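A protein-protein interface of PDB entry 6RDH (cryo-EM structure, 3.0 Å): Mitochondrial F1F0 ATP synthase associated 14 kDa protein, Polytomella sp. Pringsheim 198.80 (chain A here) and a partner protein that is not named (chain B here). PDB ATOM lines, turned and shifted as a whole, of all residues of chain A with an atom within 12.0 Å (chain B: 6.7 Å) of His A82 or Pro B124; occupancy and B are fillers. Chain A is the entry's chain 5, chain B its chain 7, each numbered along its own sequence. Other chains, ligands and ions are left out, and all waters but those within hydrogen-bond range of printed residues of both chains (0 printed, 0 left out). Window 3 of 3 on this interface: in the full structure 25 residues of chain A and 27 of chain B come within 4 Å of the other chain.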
ATOM      1  N   LYS A  73      38.083 -13.078   2.137  1.00  0.00           N
ATOM      2  CA  LYS A  73      37.544 -13.425   0.829  1.00  0.00           C
ATOM      3  C   LYS A  73      36.722 -14.699   0.907  1.00  0.00           C
ATOM      4  O   LYS A  73      35.734 -14.847   0.183  1.00  0.00           O
ATOM      5  CB  LYS A  73      38.688 -13.568  -0.171  1.00  0.00           C
ATOM      6  CG  LYS A  73      38.285 -13.898  -1.590  1.00  0.00           C
ATOM      7  CD  LYS A  73      37.415 -12.820  -2.195  1.00  0.00           C
ATOM      8  CE  LYS A  73      37.096 -13.140  -3.641  1.00  0.00           C
ATOM      9  NZ  LYS A  73      36.322 -12.060  -4.292  1.00  0.00           N
ATOM     10  N   ASN A  74      37.100 -15.606   1.804  1.00  0.00           N
ATOM     11  CA  ASN A  74      36.330 -16.822   2.032  1.00  0.00           C
ATOM     12  C   ASN A  74      34.958 -16.510   2.609  1.00  0.00           C
ATOM     13  O   ASN A  74      33.963 -17.134   2.230  1.00  0.00           O
ATOM     14  CB  ASN A  74      37.112 -17.736   2.962  1.00  0.00           C
ATOM     15  CG  ASN A  74      36.259 -18.776   3.599  1.00  0.00           C
ATOM     16  OD1 ASN A  74      35.634 -19.575   2.918  1.00  0.00           O
ATOM     17  ND2 ASN A  74      36.224 -18.784   4.919  1.00  0.00           N
ATOM     18  N   GLN A  75      34.875 -15.524   3.499  1.00  0.00           N
ATOM     19  CA  GLN A  75      33.584 -15.153   4.058  1.00  0.00           C
ATOM     20  C   GLN A  75      32.713 -14.440   3.041  1.00  0.00           C
ATOM     21  O   GLN A  75      31.488 -14.572   3.086  1.00  0.00           O
ATOM     22  CB  GLN A  75      33.772 -14.285   5.288  1.00  0.00           C
ATOM     23  CG  GLN A  75      34.389 -15.023   6.434  1.00  0.00           C
ATOM     24  CD  GLN A  75      34.374 -14.216   7.693  1.00  0.00           C
ATOM     25  OE1 GLN A  75      33.795 -13.139   7.739  1.00  0.00           O
ATOM     26  NE2 GLN A  75      35.011 -14.729   8.727  1.00  0.00           N
ATOM     27  N   VAL A  76      33.316 -13.717   2.103  1.00  0.00           N
ATOM     28  CA  VAL A  76      32.549 -13.134   1.007  1.00  0.00           C
ATOM     29  C   VAL A  76      32.011 -14.228   0.099  1.00  0.00           C
ATOM     30  O   VAL A  76      30.838 -14.217  -0.284  1.00  0.00           O
ATOM     31  CB  VAL A  76      33.417 -12.135   0.228  1.00  0.00           C
ATOM     32  CG1 VAL A  76      32.700 -11.631  -0.993  1.00  0.00           C
ATOM     33  CG2 VAL A  76      33.757 -11.008   1.100  1.00  0.00           C
ATOM     34  N   LEU A  77      32.851 -15.205  -0.236  1.00  0.00           N
ATOM     35  CA  LEU A  77      32.416 -16.277  -1.118  1.00  0.00           C
ATOM     36  C   LEU A  77      31.426 -17.220  -0.460  1.00  0.00           C
ATOM     37  O   LEU A  77      30.717 -17.932  -1.170  1.00  0.00           O
ATOM     38  CB  LEU A  77      33.616 -17.073  -1.610  1.00  0.00           C
ATOM     39  CG  LEU A  77      34.556 -16.384  -2.586  1.00  0.00           C
ATOM     40  CD1 LEU A  77      35.436 -17.419  -3.207  1.00  0.00           C
ATOM     41  CD2 LEU A  77      33.778 -15.659  -3.648  1.00  0.00           C
ATOM     42  N   GLU A  78      31.359 -17.258   0.863  1.00  0.00           N
ATOM     43  CA  GLU A  78      30.355 -18.089   1.507  1.00  0.00           C
ATOM     44  C   GLU A  78      29.134 -17.314   1.976  1.00  0.00           C
ATOM     45  O   GLU A  78      28.130 -17.936   2.323  1.00  0.00           O
ATOM     46  CB  GLU A  78      30.964 -18.846   2.684  1.00  0.00           C
ATOM     47  CG  GLU A  78      31.003 -18.086   3.970  1.00  0.00           C
ATOM     48  CD  GLU A  78      31.643 -18.884   5.069  1.00  0.00           C
ATOM     49  OE1 GLU A  78      32.052 -20.030   4.800  1.00  0.00           O
ATOM     50  OE2 GLU A  78      31.750 -18.365   6.197  1.00  0.00           O
ATOM     51  N   ASN A  79      29.185 -15.989   2.004  1.00  0.00           N
ATOM     52  CA  ASN A  79      28.010 -15.180   2.266  1.00  0.00           C
ATOM     53  C   ASN A  79      27.387 -14.641   0.997  1.00  0.00           C
ATOM     54  O   ASN A  79      26.342 -13.999   1.062  1.00  0.00           O
ATOM     55  CB  ASN A  79      28.368 -14.023   3.195  1.00  0.00           C
ATOM     56  CG  ASN A  79      28.329 -14.410   4.645  1.00  0.00           C
ATOM     57  OD1 ASN A  79      27.270 -14.672   5.197  1.00  0.00           O
ATOM     58  ND2 ASN A  79      29.489 -14.477   5.266  1.00  0.00           N
ATOM     59  N   VAL A  80      28.015 -14.862  -0.148  1.00  0.00           N
ATOM     60  CA  VAL A  80      27.457 -14.475  -1.431  1.00  0.00           C
ATOM     61  C   VAL A  80      26.929 -15.685  -2.187  1.00  0.00           C
ATOM     62  O   VAL A  80      25.794 -15.685  -2.657  1.00  0.00           O
ATOM     63  CB  VAL A  80      28.510 -13.694  -2.247  1.00  0.00           C
ATOM     64  CG1 VAL A  80      28.207 -13.726  -3.719  1.00  0.00           C
ATOM     65  CG2 VAL A  80      28.571 -12.265  -1.770  1.00  0.00           C
ATOM     66  N   PHE A  81      27.731 -16.737  -2.294  1.00  0.00           N
ATOM     67  CA  PHE A  81      27.280 -17.995  -2.874  1.00  0.00           C
ATOM     68  C   PHE A  81      26.908 -18.964  -1.757  1.00  0.00           C
ATOM     69  O   PHE A  81      27.554 -19.982  -1.527  1.00  0.00           O
ATOM     70  CB  PHE A  81      28.355 -18.566  -3.785  1.00  0.00           C
ATOM     71  CG  PHE A  81      28.895 -17.574  -4.757  1.00  0.00           C
ATOM     72  CD1 PHE A  81      28.110 -17.107  -5.790  1.00  0.00           C
ATOM     73  CD2 PHE A  81      30.180 -17.094  -4.630  1.00  0.00           C
ATOM     74  CE1 PHE A  81      28.599 -16.185  -6.680  1.00  0.00           C
ATOM     75  CE2 PHE A  81      30.671 -16.171  -5.520  1.00  0.00           C
ATOM     76  CZ  PHE A  81      29.880 -15.721  -6.544  1.00  0.00           C
ATOM     77  N   HIS A  82      25.824 -18.624  -1.065  1.00  0.00           N
ATOM     78  CA  HIS A  82      25.468 -19.341   0.153  1.00  0.00           C
ATOM     79  C   HIS A  82      24.781 -20.665  -0.141  1.00  0.00           C
ATOM     80  O   HIS A  82      25.105 -21.684   0.477  1.00  0.00           O
ATOM     81  CB  HIS A  82      24.583 -18.468   1.037  1.00  0.00           C
ATOM     82  CG  HIS A  82      23.465 -17.796   0.305  1.00  0.00           C
ATOM     83  ND1 HIS A  82      22.194 -18.318   0.251  1.00  0.00           N
ATOM     84  CD2 HIS A  82      23.423 -16.635  -0.386  1.00  0.00           C
ATOM     85  CE1 HIS A  82      21.416 -17.509  -0.445  1.00  0.00           C
ATOM     86  NE2 HIS A  82      22.139 -16.481  -0.844  1.00  0.00           N
ATOM     87  N   THR A  83      23.834 -20.674  -1.068  1.00  0.00           N
ATOM     88  CA  THR A  83      23.070 -21.861  -1.413  1.00  0.00           C
ATOM     89  C   THR A  83      23.445 -22.272  -2.829  1.00  0.00           C
ATOM     90  O   THR A  83      23.689 -21.417  -3.680  1.00  0.00           O
ATOM     91  CB  THR A  83      21.563 -21.577  -1.308  1.00  0.00           C
ATOM     92  OG1 THR A  83      21.278 -21.014  -0.025  1.00  0.00           O
ATOM     93  CG2 THR A  83      20.742 -22.842  -1.436  1.00  0.00           C
ATOM     94  N   ALA A  84      23.533 -23.569  -3.070  1.00  0.00           N
ATOM     95  CA  ALA A  84      23.757 -24.049  -4.423  1.00  0.00           C
ATOM     96  C   ALA A  84      22.523 -23.767  -5.266  1.00  0.00           C
ATOM     97  O   ALA A  84      21.413 -24.108  -4.854  1.00  0.00           O
ATOM     98  CB  ALA A  84      24.065 -25.538  -4.411  1.00  0.00           C
ATOM     99  N   PRO A  85      22.665 -23.142  -6.427  1.00  0.00           N
ATOM    100  CA  PRO A  85      21.486 -22.697  -7.171  1.00  0.00           C
ATOM    101  C   PRO A  85      20.779 -23.840  -7.881  1.00  0.00           C
ATOM    102  O   PRO A  85      21.371 -24.868  -8.214  1.00  0.00           O
ATOM    103  CB  PRO A  85      22.066 -21.698  -8.176  1.00  0.00           C
ATOM    104  CG  PRO A  85      23.440 -22.167  -8.391  1.00  0.00           C
ATOM    105  CD  PRO A  85      23.915 -22.766  -7.099  1.00  0.00           C
ATOM    106  N   LYS A  86      19.481 -23.647  -8.098  1.00  0.00           N
ATOM    107  CA  LYS A  86      18.663 -24.656  -8.748  1.00  0.00           C
ATOM    108  C   LYS A  86      18.881 -24.604 -10.247  1.00  0.00           C
ATOM    109  O   LYS A  86      18.773 -23.538 -10.858  1.00  0.00           O
ATOM    110  CB  LYS A  86      17.190 -24.445  -8.426  1.00  0.00           C
ATOM    111  CG  LYS A  86      16.795 -24.857  -7.034  1.00  0.00           C
ATOM    112  CD  LYS A  86      16.498 -26.325  -6.959  1.00  0.00           C
ATOM    113  CE  LYS A  86      15.872 -26.670  -5.634  1.00  0.00           C
ATOM    114  NZ  LYS A  86      15.434 -28.079  -5.600  1.00  0.00           N
ATOM    115  N   TYR B 119      17.405 -14.663  -6.529  1.00  0.00           N
ATOM    116  CA  TYR B 119      18.354 -15.252  -5.595  1.00  0.00           C
ATOM    117  C   TYR B 119      18.901 -14.201  -4.650  1.00  0.00           C
ATOM    118  O   TYR B 119      18.922 -14.397  -3.432  1.00  0.00           O
ATOM    119  CB  TYR B 119      19.492 -15.907  -6.377  1.00  0.00           C
ATOM    120  CG  TYR B 119      20.405 -16.832  -5.614  1.00  0.00           C
ATOM    121  CD1 TYR B 119      21.388 -16.337  -4.776  1.00  0.00           C
ATOM    122  CD2 TYR B 119      20.327 -18.193  -5.783  1.00  0.00           C
ATOM    123  CE1 TYR B 119      22.217 -17.163  -4.095  1.00  0.00           C
ATOM    124  CE2 TYR B 119      21.161 -19.031  -5.101  1.00  0.00           C
ATOM    125  CZ  TYR B 119      22.104 -18.503  -4.265  1.00  0.00           C
ATOM    126  OH  TYR B 119      22.954 -19.314  -3.579  1.00  0.00           O
ATOM    127  N   TYR B 120      19.370 -13.088  -5.195  1.00  0.00           N
ATOM    128  CA  TYR B 120      20.131 -12.131  -4.418  1.00  0.00           C
ATOM    129  C   TYR B 120      19.268 -11.072  -3.763  1.00  0.00           C
ATOM    130  O   TYR B 120      19.738 -10.400  -2.845  1.00  0.00           O
ATOM    131  CB  TYR B 120      21.191 -11.475  -5.299  1.00  0.00           C
ATOM    132  CG  TYR B 120      22.250 -12.448  -5.729  1.00  0.00           C
ATOM    133  CD1 TYR B 120      23.058 -13.069  -4.797  1.00  0.00           C
ATOM    134  CD2 TYR B 120      22.437 -12.751  -7.061  1.00  0.00           C
ATOM    135  CE1 TYR B 120      24.015 -13.967  -5.180  1.00  0.00           C
ATOM    136  CE2 TYR B 120      23.397 -13.647  -7.452  1.00  0.00           C
ATOM    137  CZ  TYR B 120      24.182 -14.246  -6.512  1.00  0.00           C
ATOM    138  OH  TYR B 120      25.138 -15.141  -6.907  1.00  0.00           O
ATOM    139  N   ALA B 122      16.636 -11.942  -2.086  1.00  0.00           N
ATOM    140  CA  ALA B 122      15.965 -12.630  -1.003  1.00  0.00           C
ATOM    141  C   ALA B 122      16.898 -12.884   0.166  1.00  0.00           C
ATOM    142  O   ALA B 122      18.102 -13.072  -0.005  1.00  0.00           O
ATOM    143  CB  ALA B 122      15.392 -13.956  -1.489  1.00  0.00           C
ATOM    144  N   HIS B 123      16.311 -12.874   1.356  1.00  0.00           N
ATOM    145  CA  HIS B 123      16.965 -13.322   2.572  1.00  0.00           C
ATOM    146  C   HIS B 123      17.454 -14.753   2.384  1.00  0.00           C
ATOM    147  O   HIS B 123      16.779 -15.544   1.721  1.00  0.00           O
ATOM    148  CB  HIS B 123      15.957 -13.247   3.716  1.00  0.00           C
ATOM    149  CG  HIS B 123      16.524 -13.482   5.077  1.00  0.00           C
ATOM    150  ND1 HIS B 123      16.627 -12.483   6.015  1.00  0.00           N
ATOM    151  CD2 HIS B 123      16.956 -14.611   5.683  1.00  0.00           C
ATOM    152  CE1 HIS B 123      17.128 -12.978   7.130  1.00  0.00           C
ATOM    153  NE2 HIS B 123      17.340 -14.268   6.954  1.00  0.00           N
ATOM    154  N   PRO B 124      18.629 -15.106   2.912  1.00  0.00           N
ATOM    155  CA  PRO B 124      19.171 -16.453   2.662  1.00  0.00           C
ATOM    156  C   PRO B 124      18.338 -17.585   3.230  1.00  0.00           C
ATOM    157  O   PRO B 124      18.178 -18.615   2.567  1.00  0.00           O
ATOM    158  CB  PRO B 124      20.550 -16.387   3.323  1.00  0.00           C
ATOM    159  CG  PRO B 124      20.903 -14.959   3.271  1.00  0.00           C
ATOM    160  CD  PRO B 124      19.645 -14.207   3.478  1.00  0.00           C
ATOM    161  N   GLU B 125      17.782 -17.417   4.426  1.00  0.00           N
ATOM    162  CA  GLU B 125      16.974 -18.478   5.009  1.00  0.00           C
ATOM    163  C   GLU B 125      15.641 -18.629   4.295  1.00  0.00           C
ATOM    164  O   GLU B 125      15.123 -19.746   4.191  1.00  0.00           O
ATOM    165  CB  GLU B 125      16.765 -18.216   6.493  1.00  0.00           C
ATOM    166  CG  GLU B 125      18.070 -18.052   7.244  1.00  0.00           C
ATOM    167  CD  GLU B 125      18.994 -19.251   7.087  1.00  0.00           C
ATOM    168  OE1 GLU B 125      18.530 -20.394   7.273  1.00  0.00           O
ATOM    169  OE2 GLU B 125      20.186 -19.051   6.777  1.00  0.00           O
ATOM    170  N   ASP B 126      15.096 -17.541   3.755  1.00  0.00           N
ATOM    171  CA  ASP B 126      13.875 -17.660   2.972  1.00  0.00           C
ATOM    172  C   ASP B 126      14.132 -18.328   1.633  1.00  0.00           C
ATOM    173  O   ASP B 126      13.288 -19.088   1.158  1.00  0.00           O
ATOM    174  CB  ASP B 126      13.237 -16.293   2.776  1.00  0.00           C
ATOM    175  CG  ASP B 126      12.673 -15.741   4.055  1.00  0.00           C
ATOM    176  OD1 ASP B 126      12.422 -16.539   4.976  1.00  0.00           O
ATOM    177  OD2 ASP B 126      12.477 -14.515   4.146  1.00  0.00           O
ATOM    178  N   LEU B 127      15.291 -18.097   1.028  1.00  0.00           N
ATOM    179  CA  LEU B 127      15.614 -18.816  -0.195  1.00  0.00           C
ATOM    180  C   LEU B 127      15.894 -20.289   0.072  1.00  0.00           C
ATOM    181  O   LEU B 127      15.564 -21.140  -0.761  1.00  0.00           O
ATOM    182  CB  LEU B 127      16.817 -18.184  -0.877  1.00  0.00           C
ATOM    183  CG  LEU B 127      16.951 -18.619  -2.323  1.00  0.00           C
ATOM    184  CD1 LEU B 127      15.981 -17.834  -3.162  1.00  0.00           C
ATOM    185  CD2 LEU B 127      18.348 -18.461  -2.801  1.00  0.00           C
ATOM    186  N   LYS B 128      16.474 -20.614   1.225  1.00  0.00           N
ATOM    187  CA  LYS B 128      16.653 -22.016   1.580  1.00  0.00           C
ATOM    188  C   LYS B 128      15.315 -22.697   1.834  1.00  0.00           C
ATOM    189  O   LYS B 128      15.115 -23.851   1.437  1.00  0.00           O
ATOM    190  CB  LYS B 128      17.558 -22.129   2.798  1.00  0.00           C
ATOM    191  CG  LYS B 128      19.000 -21.817   2.482  1.00  0.00           C
ATOM    192  CD  LYS B 128      19.922 -22.153   3.625  1.00  0.00           C
ATOM    193  CE  LYS B 128      21.357 -21.955   3.202  1.00  0.00           C
ATOM    194  NZ  LYS B 128      21.578 -20.558   2.764  1.00  0.00           N
ATOM    195  N   LYS B 129      14.375 -21.983   2.459  1.00  0.00           N
ATOM    196  CA  LYS B 129      13.024 -22.508   2.632  1.00  0.00           C
ATOM    197  C   LYS B 129      12.312 -22.675   1.299  1.00  0.00           C
ATOM    198  O   LYS B 129      11.558 -23.632   1.112  1.00  0.00           O
ATOM    199  CB  LYS B 129      12.219 -21.594   3.548  1.00  0.00           C
ATOM    200  CG  LYS B 129      12.530 -21.787   5.009  1.00  0.00           C
ATOM    201  CD  LYS B 129      11.838 -20.751   5.865  1.00  0.00           C
ATOM    202  CE  LYS B 129      12.322 -20.827   7.298  1.00  0.00           C
ATOM    203  NZ  LYS B 129      11.888 -19.652   8.090  1.00  0.00           N
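A ring nitrogen (ND1) of His A82 sits at hydrogen-bond distance from the side-chain amino group of Lys B128 (3.4 Å).
The side-chain hydroxyl (OG1) of Thr A83 lies within hydrogen-bond range of the side-chain amino group (NZ) of Lys B128 (2.8 Å).
N of Thr A83 lies within hydrogen-bond range of OH of Tyr B119 (3.0 Å).
The side-chain hydroxyl of Thr A83 lies within hydrogen-bond range of a ring nitrogen (ND1) of His A82, at 2.9 Å.
Among the printed residues, merely in contact across the chains: Val A80 with Tyr B120 (3.5 Å), Phe A81 with Tyr B120 (3.6 Å), His A82 with Tyr B119 (3.3 Å), His A82 with Pro B124 (3.98 Å) and His A82 with Leu B127 (3.98 Å).
Of the printed residues of chain B, Val A80 touches Tyr B120 (3.5 Å).
Of the printed residues of chain B, Phe A81 touches Tyr B120 (3.6 Å).
Printed residues of chain B within 4 Å of His A82: Tyr B119 (3.3 Å), Pro B124 (3.98 Å), Leu B127 (3.98 Å) and Lys B128 (3.4 Å).
Of chain A, only His A82 and Thr A83 come within 4 Å of Tyr B119.
Tyr B120 touches two residues of chain A.
No residue of chain A comes within 4 Å of His B123.
Pro B124 touches just one residue of chain A: His A82 (3.98 Å).
No residue of chain A comes within 4 Å of Glu B125.
No residue of chain A comes within 4 Å of Asp B126.
Printed residues of chain A within 4 Å of Leu B127: His A82 (3.98 Å).
The nearest residue of chain A that does not touch Pro B124 is Thr A83 (4.7 Å).
Printed residues of chain B that touch a printed residue of chain A: Tyr B119, Tyr B120, Pro B124, Leu B127 and Lys B128.
Hydrophobic or aromatic side chains of chain B within 4 Å of the printed part of chain A: Tyr B119, Tyr B120, Pro B124 and Leu B127.
Of the 14 printed residues of chain A, 4 touch a printed residue of chain B.
Printed residues of chain A that touch a printed residue of chain B: Val A80, Phe A81, His A82 and Thr A83.
Among the printed residues, 8 pairs touch across the chains.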
